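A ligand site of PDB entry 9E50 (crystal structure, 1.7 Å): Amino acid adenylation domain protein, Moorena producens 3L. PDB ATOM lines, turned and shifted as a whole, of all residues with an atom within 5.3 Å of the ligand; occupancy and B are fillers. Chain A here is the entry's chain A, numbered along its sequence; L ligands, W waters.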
ATOM      1  N   TYR A  32      27.570  -1.551 -15.904  1.00  0.00           N
ATOM      2  CA  TYR A  32      28.830  -2.119 -16.346  1.00  0.00           C
ATOM      3  C   TYR A  32      28.734  -3.640 -16.190  1.00  0.00           C
ATOM      4  O   TYR A  32      27.717  -4.165 -15.715  1.00  0.00           O
ATOM      5  CB  TYR A  32      30.005  -1.526 -15.561  1.00  0.00           C
ATOM      6  CG  TYR A  32      29.743  -1.445 -14.082  1.00  0.00           C
ATOM      7  CD1 TYR A  32      29.989  -2.522 -13.248  1.00  0.00           C
ATOM      8  CD2 TYR A  32      29.215  -0.288 -13.505  1.00  0.00           C
ATOM      9  CE1 TYR A  32      29.731  -2.456 -11.882  1.00  0.00           C
ATOM     10  CE2 TYR A  32      28.954  -0.206 -12.157  1.00  0.00           C
ATOM     11  CZ  TYR A  32      29.211  -1.297 -11.348  1.00  0.00           C
ATOM     12  OH  TYR A  32      28.948  -1.224  -9.997  1.00  0.00           O
ATOM     13  N   TYR A  83      37.702   2.138 -11.213  1.00  0.00           N
ATOM     14  CA  TYR A  83      38.516   2.629 -10.111  1.00  0.00           C
ATOM     15  C   TYR A  83      39.974   2.799 -10.502  1.00  0.00           C
ATOM     16  O   TYR A  83      40.656   3.676  -9.959  1.00  0.00           O
ATOM     17  CB  TYR A  83      38.410   1.677  -8.926  1.00  0.00           C
ATOM     18  CG  TYR A  83      37.161   1.809  -8.086  1.00  0.00           C
ATOM     19  CD1 TYR A  83      36.900   2.965  -7.361  1.00  0.00           C
ATOM     20  CD2 TYR A  83      36.258   0.746  -7.971  1.00  0.00           C
ATOM     21  CE1 TYR A  83      35.768   3.077  -6.559  1.00  0.00           C
ATOM     22  CE2 TYR A  83      35.126   0.854  -7.179  1.00  0.00           C
ATOM     23  CZ  TYR A  83      34.891   2.015  -6.476  1.00  0.00           C
ATOM     24  OH  TYR A  83      33.768   2.124  -5.673  1.00  0.00           O
ATOM     25  N   THR A 111      24.588   4.191 -12.363  1.00  0.00           N
ATOM     26  CA  THR A 111      24.207   3.149 -11.416  1.00  0.00           C
ATOM     27  C   THR A 111      25.427   2.489 -10.782  1.00  0.00           C
ATOM     28  O   THR A 111      26.575   2.710 -11.181  1.00  0.00           O
ATOM     29  CB  THR A 111      23.347   2.058 -12.095  1.00  0.00           C
ATOM     30  OG1 THR A 111      24.176   1.218 -12.924  1.00  0.00           O
ATOM     31  CG2 THR A 111      22.225   2.683 -12.927  1.00  0.00           C
ATOM     32  N   GLY A 112      25.153   1.665  -9.771  1.00  0.00           N
ATOM     33  CA  GLY A 112      26.197   0.878  -9.146  1.00  0.00           C
ATOM     34  C   GLY A 112      27.286   1.750  -8.544  1.00  0.00           C
ATOM     35  O   GLY A 112      27.025   2.770  -7.901  1.00  0.00           O
ATOM     36  N   LEU A 113      28.535   1.354  -8.798  1.00  0.00           N
ATOM     37  CA  LEU A 113      29.680   2.046  -8.234  1.00  0.00           C
ATOM     38  C   LEU A 113      30.242   3.117  -9.160  1.00  0.00           C
ATOM     39  O   LEU A 113      31.330   3.638  -8.885  1.00  0.00           O
ATOM     40  CB  LEU A 113      30.776   1.041  -7.871  1.00  0.00           C
ATOM     41  CG  LEU A 113      30.479   0.273  -6.581  1.00  0.00           C
ATOM     42  CD1 LEU A 113      31.502  -0.819  -6.349  1.00  0.00           C
ATOM     43  CD2 LEU A 113      30.429   1.245  -5.402  1.00  0.00           C
ATOM     44  N   PRO A 115      29.214   6.305  -9.522  1.00  0.00           N
ATOM     45  CA  PRO A 115      29.470   7.526  -8.728  1.00  0.00           C
ATOM     46  C   PRO A 115      30.678   7.389  -7.798  1.00  0.00           C
ATOM     47  O   PRO A 115      31.544   8.274  -7.772  1.00  0.00           O
ATOM     48  CB  PRO A 115      28.161   7.709  -7.947  1.00  0.00           C
ATOM     49  CG  PRO A 115      27.115   7.137  -8.853  1.00  0.00           C
ATOM     50  CD  PRO A 115      27.790   5.919  -9.461  1.00  0.00           C
ATOM     51  N   SER A 116      30.777   6.283  -7.068  1.00  0.00           N
ATOM     52  CA  SER A 116      31.890   6.091  -6.153  1.00  0.00           C
ATOM     53  C   SER A 116      33.241   6.210  -6.856  1.00  0.00           C
ATOM     54  O   SER A 116      34.222   6.656  -6.249  1.00  0.00           O
ATOM     55  CB  SER A 116      31.764   4.719  -5.474  1.00  0.00           C
ATOM     56  OG  SER A 116      32.803   4.489  -4.546  1.00  0.00           O
ATOM     57  N   TYR A 120      31.606  10.940  -7.513  1.00  0.00           N
ATOM     58  CA  TYR A 120      30.146  11.025  -7.463  1.00  0.00           C
ATOM     59  C   TYR A 120      29.603  11.875  -8.609  1.00  0.00           C
ATOM     60  O   TYR A 120      28.651  12.646  -8.446  1.00  0.00           O
ATOM     61  CB  TYR A 120      29.677  11.500  -6.092  1.00  0.00           C
ATOM     62  CG  TYR A 120      30.224  10.565  -5.038  1.00  0.00           C
ATOM     63  CD1 TYR A 120      29.610   9.330  -4.787  1.00  0.00           C
ATOM     64  CD2 TYR A 120      31.407  10.857  -4.373  1.00  0.00           C
ATOM     65  CE1 TYR A 120      30.150   8.445  -3.865  1.00  0.00           C
ATOM     66  CE2 TYR A 120      31.950   9.984  -3.446  1.00  0.00           C
ATOM     67  CZ  TYR A 120      31.312   8.778  -3.198  1.00  0.00           C
ATOM     68  OH  TYR A 120      31.879   7.918  -2.274  1.00  0.00           O
ATOM     69  N   HIS A 141      21.135   9.052  -6.125  1.00  0.00           N
ATOM     70  CA  HIS A 141      21.236   8.498  -4.773  1.00  0.00           C
ATOM     71  C   HIS A 141      20.133   8.984  -3.838  1.00  0.00           C
ATOM     72  O   HIS A 141      19.883   8.351  -2.812  1.00  0.00           O
ATOM     73  CB  HIS A 141      22.611   8.800  -4.178  1.00  0.00           C
ATOM     74  CG  HIS A 141      23.694   7.940  -4.753  1.00  0.00           C
ATOM     75  ND1 HIS A 141      24.999   8.010  -4.334  1.00  0.00           N
ATOM     76  CD2 HIS A 141      23.655   7.004  -5.724  1.00  0.00           C
ATOM     77  CE1 HIS A 141      25.717   7.124  -5.008  1.00  0.00           C
ATOM     78  NE2 HIS A 141      24.925   6.511  -5.869  1.00  0.00           N
ATOM     79  N   THR A 144      17.555   6.366  -4.598  1.00  0.00           N
ATOM     80  CA  THR A 144      18.017   5.135  -3.967  1.00  0.00           C
ATOM     81  C   THR A 144      17.818   5.194  -2.464  1.00  0.00           C
ATOM     82  O   THR A 144      17.354   4.218  -1.857  1.00  0.00           O
ATOM     83  CB  THR A 144      19.498   4.906  -4.292  1.00  0.00           C
ATOM     84  OG1 THR A 144      19.654   4.744  -5.698  1.00  0.00           O
ATOM     85  CG2 THR A 144      20.013   3.664  -3.565  1.00  0.00           C
ATOM     86  N   ILE A 171      26.007  -0.471   7.869  1.00  0.00           N
ATOM     87  CA  ILE A 171      27.286  -0.956   7.371  1.00  0.00           C
ATOM     88  C   ILE A 171      27.581  -0.197   6.085  1.00  0.00           C
ATOM     89  O   ILE A 171      26.975  -0.480   5.046  1.00  0.00           O
ATOM     90  CB  ILE A 171      27.276  -2.467   7.102  1.00  0.00           C
ATOM     91  CG1 ILE A 171      26.810  -3.236   8.339  1.00  0.00           C
ATOM     92  CG2 ILE A 171      28.660  -2.920   6.651  1.00  0.00           C
ATOM     93  CD1 ILE A 171      26.841  -4.744   8.136  1.00  0.00           C
ATOM     94  N   GLY A 172      28.512   0.758   6.139  1.00  0.00           N
ATOM     95  CA  GLY A 172      28.834   1.529   4.958  1.00  0.00           C
ATOM     96  C   GLY A 172      28.141   2.872   4.931  1.00  0.00           C
ATOM     97  O   GLY A 172      26.973   2.975   4.520  1.00  0.00           O
ATOM     98  N   LEU A 173      28.841   3.918   5.379  1.00  0.00           N
ATOM     99  CA  LEU A 173      28.235   5.243   5.430  1.00  0.00           C
ATOM    100  C   LEU A 173      28.859   6.140   4.376  1.00  0.00           C
ATOM    101  O   LEU A 173      29.427   7.197   4.692  1.00  0.00           O
ATOM    102  CB  LEU A 173      28.384   5.827   6.834  1.00  0.00           C
ATOM    103  CG  LEU A 173      27.387   5.112   7.764  1.00  0.00           C
ATOM    104  CD1 LEU A 173      27.787   5.223   9.205  1.00  0.00           C
ATOM    105  CD2 LEU A 173      25.972   5.618   7.557  1.00  0.00           C
ATOM    106  N   GLY A 174      28.757   5.717   3.123  1.00  0.00           N
ATOM    107  CA  GLY A 174      29.182   6.524   1.998  1.00  0.00           C
ATOM    108  C   GLY A 174      28.041   7.360   1.466  1.00  0.00           C
ATOM    109  O   GLY A 174      27.195   7.839   2.233  1.00  0.00           O
ATOM    110  N   SER A 175      27.983   7.527   0.144  1.00  0.00           N
ATOM    111  CA  SER A 175      26.966   8.398  -0.451  1.00  0.00           C
ATOM    112  C   SER A 175      25.559   7.890  -0.182  1.00  0.00           C
ATOM    113  O   SER A 175      24.698   8.626   0.319  1.00  0.00           O
ATOM    114  CB  SER A 175      27.214   8.543  -1.942  1.00  0.00           C
ATOM    115  OG  SER A 175      26.194   9.302  -2.564  1.00  0.00           O
ATOM    116  N   VAL A 176      25.310   6.613  -0.481  1.00  0.00           N
ATOM    117  CA  VAL A 176      23.971   6.055  -0.252  1.00  0.00           C
ATOM    118  C   VAL A 176      23.668   5.983   1.237  1.00  0.00           C
ATOM    119  O   VAL A 176      22.590   6.406   1.687  1.00  0.00           O
ATOM    120  CB  VAL A 176      23.835   4.685  -0.929  1.00  0.00           C
ATOM    121  CG1 VAL A 176      22.554   4.008  -0.481  1.00  0.00           C
ATOM    122  CG2 VAL A 176      23.830   4.843  -2.452  1.00  0.00           C
ATOM    123  N   GLY A 177      24.588   5.441   2.032  1.00  0.00           N
ATOM    124  CA  GLY A 177      24.337   5.279   3.453  1.00  0.00           C
ATOM    125  C   GLY A 177      23.962   6.581   4.141  1.00  0.00           C
ATOM    126  O   GLY A 177      23.067   6.619   4.978  1.00  0.00           O
ATOM    127  N   CYS A 197      28.917   1.712  11.255  1.00  0.00           N
ATOM    128  CA  CYS A 197      30.036   0.831  10.931  1.00  0.00           C
ATOM    129  C   CYS A 197      30.645   1.232   9.600  1.00  0.00           C
ATOM    130  O   CYS A 197      29.957   1.253   8.577  1.00  0.00           O
ATOM    131  CB  CYS A 197      29.599  -0.635  10.900  1.00  0.00           C
ATOM    132  SG  CYS A 197      30.904  -1.759  10.354  1.00  0.00           S
ATOM    133  N   ASP A 198      31.941   1.532   9.613  1.00  0.00           N
ATOM    134  CA  ASP A 198      32.719   1.773   8.407  1.00  0.00           C
ATOM    135  C   ASP A 198      34.177   1.469   8.725  1.00  0.00           C
ATOM    136  O   ASP A 198      34.487   0.939   9.806  1.00  0.00           O
ATOM    137  CB  ASP A 198      32.518   3.208   7.899  1.00  0.00           C
ATOM    138  CG  ASP A 198      32.658   3.325   6.392  1.00  0.00           C
ATOM    139  OD1 ASP A 198      33.744   2.971   5.868  1.00  0.00           O
ATOM    140  OD2 ASP A 198      31.682   3.736   5.727  1.00  0.00           O
ATOM    141  N   VAL A 199      35.073   1.788   7.798  1.00  0.00           N
ATOM    142  CA  VAL A 199      36.477   1.413   7.959  1.00  0.00           C
ATOM    143  C   VAL A 199      37.185   2.351   8.936  1.00  0.00           C
ATOM    144  O   VAL A 199      36.695   3.421   9.281  1.00  0.00           O
ATOM    145  CB  VAL A 199      37.195   1.391   6.591  1.00  0.00           C
ATOM    146  CG1 VAL A 199      36.571   0.331   5.683  1.00  0.00           C
ATOM    147  CG2 VAL A 199      37.130   2.769   5.941  1.00  0.00           C
ATOM    148  N   LYS A 202      37.775   6.138   8.606  1.00  0.00           N
ATOM    149  CA  LYS A 202      36.625   7.011   8.670  1.00  0.00           C
ATOM    150  C   LYS A 202      36.126   7.235  10.094  1.00  0.00           C
ATOM    151  O   LYS A 202      34.999   7.700  10.282  1.00  0.00           O
ATOM    152  CB  LYS A 202      35.491   6.480   7.795  1.00  0.00           C
ATOM    153  CG  LYS A 202      35.878   6.364   6.328  1.00  0.00           C
ATOM    154  CD  LYS A 202      34.669   6.463   5.414  1.00  0.00           C
ATOM    155  CE  LYS A 202      35.080   6.489   3.953  1.00  0.00           C
ATOM    156  NZ  LYS A 202      33.902   6.639   3.051  1.00  0.00           N
ATOM    157  N   SER A 228      35.413  -1.430  10.995  1.00  0.00           N
ATOM    158  CA  SER A 228      35.744  -2.644  10.267  1.00  0.00           C
ATOM    159  C   SER A 228      37.217  -2.658   9.881  1.00  0.00           C
ATOM    160  O   SER A 228      37.811  -1.618   9.582  1.00  0.00           O
ATOM    161  CB  SER A 228      34.915  -2.776   8.985  1.00  0.00           C
ATOM    162  OG  SER A 228      33.549  -2.986   9.268  1.00  0.00           O
ATOM    163  N   LYS A 229      37.795  -3.851   9.879  1.00  0.00           N
ATOM    164  CA  LYS A 229      39.079  -4.082   9.237  1.00  0.00           C
ATOM    165  C   LYS A 229      38.845  -4.789   7.904  1.00  0.00           C
ATOM    166  O   LYS A 229      38.418  -4.148   6.942  1.00  0.00           O
ATOM    167  CB  LYS A 229      40.008  -4.880  10.155  1.00  0.00           C
ATOM    168  CG  LYS A 229      40.158  -4.258  11.543  1.00  0.00           C
ATOM    169  CD  LYS A 229      40.959  -5.175  12.484  1.00  0.00           C
ATOM    170  CE  LYS A 229      40.976  -4.641  13.912  1.00  0.00           C
ATOM    171  NZ  LYS A 229      41.741  -5.539  14.843  1.00  0.00           N
ATOM    172  N   THR A 230      39.093  -6.096   7.834  1.00  0.00           N
ATOM    173  CA  THR A 230      38.729  -6.824   6.622  1.00  0.00           C
ATOM    174  C   THR A 230      37.275  -7.277   6.634  1.00  0.00           C
ATOM    175  O   THR A 230      36.701  -7.538   5.566  1.00  0.00           O
ATOM    176  CB  THR A 230      39.639  -8.043   6.411  1.00  0.00           C
ATOM    177  OG1 THR A 230      39.408  -9.029   7.418  1.00  0.00           O
ATOM    178  CG2 THR A 230      41.109  -7.624   6.437  1.00  0.00           C
ATOM    179  N   THR A 231      36.660  -7.389   7.815  1.00  0.00           N
ATOM    180  CA  THR A 231      35.241  -7.699   7.953  1.00  0.00           C
ATOM    181  C   THR A 231      34.651  -6.817   9.041  1.00  0.00           C
ATOM    182  O   THR A 231      35.378  -6.111   9.749  1.00  0.00           O
ATOM    183  CB  THR A 231      35.004  -9.172   8.277  1.00  0.00           C
ATOM    184  OG1 THR A 231      35.706  -9.519   9.476  1.00  0.00           O
ATOM    185  CG2 THR A 231      35.483 -10.074   7.136  1.00  0.00           C
ATOM    186  N   VAL A 232      33.340  -6.863   9.190  1.00  0.00           N
ATOM    187  CA  VAL A 232      32.674  -6.070  10.224  1.00  0.00           C
ATOM    188  C   VAL A 232      33.103  -6.601  11.586  1.00  0.00           C
ATOM    189  O   VAL A 232      33.418  -7.785  11.728  1.00  0.00           O
ATOM    190  CB  VAL A 232      31.147  -6.091  10.076  1.00  0.00           C
ATOM    191  CG1 VAL A 232      30.734  -5.474   8.744  1.00  0.00           C
ATOM    192  CG2 VAL A 232      30.614  -7.513  10.185  1.00  0.00           C
ATOM    193  N   ALA A 245      25.292  -0.630   2.737  1.00  0.00           N
ATOM    194  CA  ALA A 245      25.598   0.151   1.540  1.00  0.00           C
ATOM    195  C   ALA A 245      27.106   0.266   1.384  1.00  0.00           C
ATOM    196  O   ALA A 245      27.653   1.379   1.411  1.00  0.00           O
ATOM    197  CB  ALA A 245      24.929   1.522   1.600  1.00  0.00           C
ATOM    198  N   THR A 246      27.797  -0.864   1.241  1.00  0.00           N
ATOM    199  CA  THR A 246      29.244  -0.885   1.119  1.00  0.00           C
ATOM    200  C   THR A 246      29.660  -0.879  -0.334  1.00  0.00           C
ATOM    201  O   THR A 246      28.874  -1.130  -1.244  1.00  0.00           O
ATOM    202  CB  THR A 246      29.832  -2.130   1.785  1.00  0.00           C
ATOM    203  OG1 THR A 246      29.534  -3.276   0.978  1.00  0.00           O
ATOM    204  CG2 THR A 246      29.257  -2.314   3.176  1.00  0.00           C
ATOM    205  N   ASN A 247      30.948  -0.613  -0.570  1.00  0.00           N
ATOM    206  CA  ASN A 247      31.552  -0.877  -1.872  1.00  0.00           C
ATOM    207  C   ASN A 247      32.499  -2.069  -1.830  1.00  0.00           C
ATOM    208  O   ASN A 247      33.356  -2.202  -2.704  1.00  0.00           O
ATOM    209  CB  ASN A 247      32.278   0.367  -2.394  1.00  0.00           C
ATOM    210  CG  ASN A 247      33.505   0.733  -1.573  1.00  0.00           C
ATOM    211  OD1 ASN A 247      33.569   0.468  -0.371  1.00  0.00           O
ATOM    212  ND2 ASN A 247      34.493   1.353  -2.222  1.00  0.00           N
ATOM    213  N   VAL A 248      32.350  -2.932  -0.817  1.00  0.00           N
ATOM    214  CA  VAL A 248      33.161  -4.138  -0.668  1.00  0.00           C
ATOM    215  C   VAL A 248      32.227  -5.311  -0.353  1.00  0.00           C
ATOM    216  O   VAL A 248      31.399  -5.206   0.557  1.00  0.00           O
ATOM    217  CB  VAL A 248      34.224  -3.987   0.434  1.00  0.00           C
ATOM    218  CG1 VAL A 248      34.977  -5.290   0.655  1.00  0.00           C
ATOM    219  CG2 VAL A 248      35.203  -2.863   0.089  1.00  0.00           C
ATOM    220  N   VAL A 251      31.589  -8.571   3.558  1.00  0.00           N
ATOM    221  CA  VAL A 251      32.177  -8.122   4.817  1.00  0.00           C
ATOM    222  C   VAL A 251      31.318  -8.489   6.008  1.00  0.00           C
ATOM    223  O   VAL A 251      31.763  -8.357   7.157  1.00  0.00           O
ATOM    224  CB  VAL A 251      32.438  -6.592   4.810  1.00  0.00           C
ATOM    225  CG1 VAL A 251      33.484  -6.258   3.764  1.00  0.00           C
ATOM    226  CG2 VAL A 251      31.140  -5.841   4.523  1.00  0.00           C
ATOM    227  N   ASP A 266      21.661  -2.458  -0.004  1.00  0.00           N
ATOM    228  CA  ASP A 266      21.795  -1.866  -1.326  1.00  0.00           C
ATOM    229  C   ASP A 266      23.152  -2.145  -1.975  1.00  0.00           C
ATOM    230  O   ASP A 266      23.335  -1.835  -3.149  1.00  0.00           O
ATOM    231  CB  ASP A 266      21.558  -0.345  -1.251  1.00  0.00           C
ATOM    232  CG  ASP A 266      21.390   0.300  -2.625  1.00  0.00           C
ATOM    233  OD1 ASP A 266      20.571  -0.185  -3.445  1.00  0.00           O
ATOM    234  OD2 ASP A 266      22.076   1.316  -2.885  1.00  0.00           O
ATOM    235  N   SER A 267      24.079  -2.735  -1.236  1.00  0.00           N
ATOM    236  CA  SER A 267      25.393  -3.043  -1.798  1.00  0.00           C
ATOM    237  C   SER A 267      25.255  -3.958  -3.013  1.00  0.00           C
ATOM    238  O   SER A 267      24.487  -4.933  -3.016  1.00  0.00           O
ATOM    239  CB  SER A 267      26.291  -3.706  -0.744  1.00  0.00           C
ATOM    240  OG  SER A 267      26.151  -3.075   0.524  1.00  0.00           O
ATOM    241  N   GLY A 268      25.997  -3.629  -4.063  1.00  0.00           N
ATOM    242  CA  GLY A 268      26.093  -4.460  -5.247  1.00  0.00           C
ATOM    243  C   GLY A 268      27.528  -4.522  -5.723  1.00  0.00           C
ATOM    244  O   GLY A 268      28.080  -3.522  -6.204  1.00  0.00           O
ATOM    245  N   PRO A 269      28.190  -5.688  -5.567  1.00  0.00           N
ATOM    246  CA  PRO A 269      27.682  -6.951  -5.003  1.00  0.00           C
ATOM    247  C   PRO A 269      27.338  -6.823  -3.527  1.00  0.00           C
ATOM    248  O   PRO A 269      27.762  -5.886  -2.851  1.00  0.00           O
ATOM    249  CB  PRO A 269      28.856  -7.922  -5.229  1.00  0.00           C
ATOM    250  CG  PRO A 269      30.064  -7.048  -5.265  1.00  0.00           C
ATOM    251  CD  PRO A 269      29.610  -5.787  -5.953  1.00  0.00           C
ATOM    252  N   MET A 332      14.694  -0.346 -10.428  1.00  0.00           N
ATOM    253  CA  MET A 332      15.669   0.146  -9.470  1.00  0.00           C
ATOM    254  C   MET A 332      15.503   1.646  -9.282  1.00  0.00           C
ATOM    255  O   MET A 332      15.234   2.387 -10.234  1.00  0.00           O
ATOM    256  CB  MET A 332      17.088  -0.180  -9.941  1.00  0.00           C
ATOM    257  CG  MET A 332      17.499  -1.621  -9.691  1.00  0.00           C
ATOM    258  SD  MET A 332      17.411  -2.121  -7.948  1.00  0.00           S
ATOM    259  CE  MET A 332      18.770  -1.199  -7.264  1.00  0.00           C
ATOM    260  N   CYS A 334      17.686   3.963  -8.491  1.00  0.00           N
ATOM    261  CA  CYS A 334      18.710   4.781  -9.126  1.00  0.00           C
ATOM    262  C   CYS A 334      18.371   5.060 -10.591  1.00  0.00           C
ATOM    263  O   CYS A 334      18.382   6.214 -11.040  1.00  0.00           O
ATOM    264  CB  CYS A 334      20.072   4.088  -9.004  1.00  0.00           C
ATOM    265  SG  CYS A 334      21.405   4.902  -9.924  1.00  0.00           S
HETATM  266  P1  LIG L   1      30.565   4.676  -1.494  1.00  0.00           P
HETATM  267  O1  LIG L   1      31.900   4.330  -2.050  1.00  0.00           O
HETATM  268  O2  LIG L   1      30.302   6.167  -1.429  1.00  0.00           O
HETATM  269  O3  LIG L   1      30.376   4.118   0.083  1.00  0.00           O
HETATM  270  C1  LIG L   1      30.777   2.729   0.342  1.00  0.00           C
HETATM  271  C2  LIG L   1      31.061   2.606   1.812  1.00  0.00           C
HETATM  272  O4  LIG L   1      31.291   1.360   2.119  1.00  0.00           O
HETATM  273  C3  LIG L   1      32.484   3.459   2.137  1.00  0.00           C
HETATM  274  O5  LIG L   1      32.179   4.447   3.184  1.00  0.00           O
HETATM  275  C4  LIG L   1      33.304   2.570   2.454  1.00  0.00           C
HETATM  276  O6  LIG L   1      34.386   3.020   3.394  1.00  0.00           O
HETATM  277  C5  LIG L   1      32.382   1.446   3.141  1.00  0.00           C
HETATM  278  N1  LIG L   1      33.025   0.318   3.345  1.00  0.00           N
HETATM  279  C6  LIG L   1      33.995  -0.264   2.619  1.00  0.00           C
HETATM  280  N2  LIG L   1      34.396  -1.394   3.257  1.00  0.00           N
HETATM  281  C7  LIG L   1      33.678  -1.494   4.384  1.00  0.00           C
HETATM  282  C8  LIG L   1      33.643  -2.520   5.529  1.00  0.00           C
HETATM  283  N3  LIG L   1      34.514  -3.697   5.549  1.00  0.00           N
HETATM  284  N4  LIG L   1      32.724  -2.325   6.613  1.00  0.00           N
HETATM  285  C9  LIG L   1      31.853  -1.190   6.655  1.00  0.00           C
HETATM  286  N5  LIG L   1      31.893  -0.234   5.562  1.00  0.00           N
HETATM  287  C10 LIG L   1      32.839  -0.436   4.428  1.00  0.00           C
HETATM  288  O7  LIG L   1      29.464   3.882  -2.404  1.00  0.00           O
HETATM  289  P2  LIG L   1      27.899   4.335  -2.609  1.00  0.00           P
HETATM  290  O8  LIG L   1      27.304   4.867  -1.336  1.00  0.00           O
HETATM  291  O9  LIG L   1      27.875   5.309  -3.790  1.00  0.00           O
HETATM  292  O10 LIG L   1      27.198   2.881  -3.032  1.00  0.00           O
HETATM  293  C11 LIG L   1      27.127   1.941  -1.981  1.00  0.00           C
HETATM  294  C12 LIG L   1      26.561   0.608  -2.525  1.00  0.00           C
HETATM  295  O11 LIG L   1      25.371   0.845  -2.984  1.00  0.00           O
HETATM  296  C13 LIG L   1      27.488   0.104  -3.747  1.00  0.00           C
HETATM  297  O12 LIG L   1      27.797  -1.322  -3.619  1.00  0.00           O
HETATM  298  C14 LIG L   1      26.789   0.372  -4.835  1.00  0.00           C
HETATM  299  O13 LIG L   1      27.069  -0.558  -5.953  1.00  0.00           O
HETATM  300  C15 LIG L   1      25.348   0.222  -4.386  1.00  0.00           C
HETATM  301  N6  LIG L   1      24.534   0.928  -5.191  1.00  0.00           N
HETATM  302  C16 LIG L   1      23.899   0.250  -6.332  1.00  0.00           C
HETATM  303  C17 LIG L   1      22.988   1.022  -7.271  1.00  0.00           C
HETATM  304  C18 LIG L   1      22.351   0.273  -8.446  1.00  0.00           C
HETATM  305  O14 LIG L   1      22.028   0.888  -9.444  1.00  0.00           O
HETATM  306  N7  LIG L   1      22.157  -1.187  -8.355  1.00  0.00           N
HETATM  307  C19 LIG L   1      22.714   2.494  -7.045  1.00  0.00           C
HETATM  308  C20 LIG L   1      23.367   3.175  -5.883  1.00  0.00           C
HETATM  309  C21 LIG L   1      24.285   2.388  -4.948  1.00  0.00           C
HETATM  310  O   HOH W   1      36.746   3.164   2.205  1.00  0.00           O
HETATM  311  O   HOH W   2      24.907   4.595  -8.170  1.00  0.00           O
HETATM  312  O   HOH W   3      34.263   5.049  -1.238  1.00  0.00           O
HETATM  313  O   HOH W   4      36.877  -3.194   3.460  1.00  0.00           O
HETATM  314  O   HOH W   5      28.481   4.778  -6.298  1.00  0.00           O
HETATM  315  O   HOH W   6      21.020  -1.825 -10.790  1.00  0.00           O
HETATM  316  O   HOH W   7      20.520   0.570  -5.899  1.00  0.00           O
HETATM  317  O   HOH W   8      27.147   4.126   1.263  1.00  0.00           O
HETATM  318  O   HOH W   9      19.786   1.215 -10.771  1.00  0.00           O
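The backbone carbonyl oxygen (O) of Asp 198 sits at hydrogen-bond distance from the backbone NH (N) of Ser 228 (2.8 Å).
The backbone NH of Thr 246 is in hydrogen-bond range of the side-chain hydroxyl of Ser 267.
The side-chain hydroxyl of Ser 116 lies within hydrogen-bond range of the side-chain hydroxyl of Tyr 83, at 2.8 Å.
The side-chain hydroxyl of Ser 228 sits at hydrogen-bond distance from the side-chain sulfur of Cys 197, 3.1 Å away.
The side-chain hydroxyl (OG) of Ser 175 sits at hydrogen-bond distance from a ring nitrogen (ND1) of His 141 (2.5 Å).
The backbone carbonyl oxygen (O) of Val 251 sits at hydrogen-bond distance from the backbone NH (N) of Val 232.
N of Ala 245 is in hydrogen-bond range of OG of Ser 267.
The backbone NH (N) of Ala 245 lies within hydrogen-bond range of the backbone carbonyl oxygen (O) of Ile 171, at 2.9 Å.
Water W5 lies within hydrogen-bond range of an oxygen (O9) of the ligand (2.6 Å), the backbone NH (N) of Ser 116 (2.9 Å) and the backbone carbonyl oxygen (O) of Gly 112 (3.0 Å).
Water W8 lies within hydrogen-bond range of O8 of the ligand (2.7 Å), O of Ala 245 (2.8 Å), N of Gly 174 (2.9 Å), N of Gly 177 (3.0 Å) and O of Gly 172 (3.5 Å).
Water W7 bridges the side-chain carboxylate of Asp 266 and a nitrogen (N7) of the ligand.
Water W2 lies within hydrogen-bond range of the backbone carbonyl oxygen of Gly 112 (2.8 Å) and a ring nitrogen (NE2) of His 141 (3.0 Å).
The side-chain carboxylate (OD2) of Asp 266 sits close to an oxygen (O11) of the ligand, at 3.3 Å.
Merely in contact with the ligand: His 141, Thr 111, Val 251, Gly 174, Ser 267, Ala 245, Met 332, Leu 113, Gly 172, Val 248, Ile 171, Cys 197, Cys 334, Val 199 and Leu 173.
Hydrophobic or aromatic side chains that line the ligand: Leu 113, Tyr 120, His 141, Ile 171, Val 176, Val 199, Val 248, Val 251 and Met 332.
Within 4 Å of the ligand: Thr 111, Gly 112, Leu 113, Ser 116, Tyr 120, His 141, Ile 171, Gly 172, Leu 173, Gly 174, Ser 175, Val 176, Cys 197, Asp 198, Val 199, Lys 202, Ser 228, Ala 245, Thr 246, Asn 247, Val 248, Val 251, Asp 266, Ser 267, Gly 268, Met 332 and Cys 334.
An oxygen (O2) of the ligand sits at hydrogen-bond distance from the side-chain hydroxyl (OH) of Tyr 120 (2.5 Å).
OD1 of Asp 198 lies within hydrogen-bond range of O6 of the ligand, at 2.6 Å.
O of Thr 246 is in hydrogen-bond range of O12 of the ligand, at 2.6 Å.
The side-chain hydroxyl (OG) of Ser 116 sits at hydrogen-bond distance from an oxygen (O1) of the ligand (2.7 Å).
The backbone NH (N) of Val 176 is in hydrogen-bond range of an oxygen (O8) of the ligand (2.8 Å).
NZ of Lys 202 sits at hydrogen-bond distance from O5 of the ligand, at 2.8 Å.
OG of Ser 228 sits at hydrogen-bond distance from N4 of the ligand (2.9 Å).
N of Gly 268 sits at hydrogen-bond distance from O12 of the ligand.
An oxygen (O13) of the ligand sits at hydrogen-bond distance from the backbone carbonyl oxygen (O) of Gly 268.
An oxygen (O4) of the ligand sits at hydrogen-bond distance from the backbone NH (N) of Asn 247.
An oxygen (O4) of the ligand sits close to the side-chain amide oxygen (OD1) of Asn 247.
N of Ser 175 lies within hydrogen-bond range of O2 of the ligand (3.1 Å).
N of Gly 112 sits at hydrogen-bond distance from O14 of the ligand.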
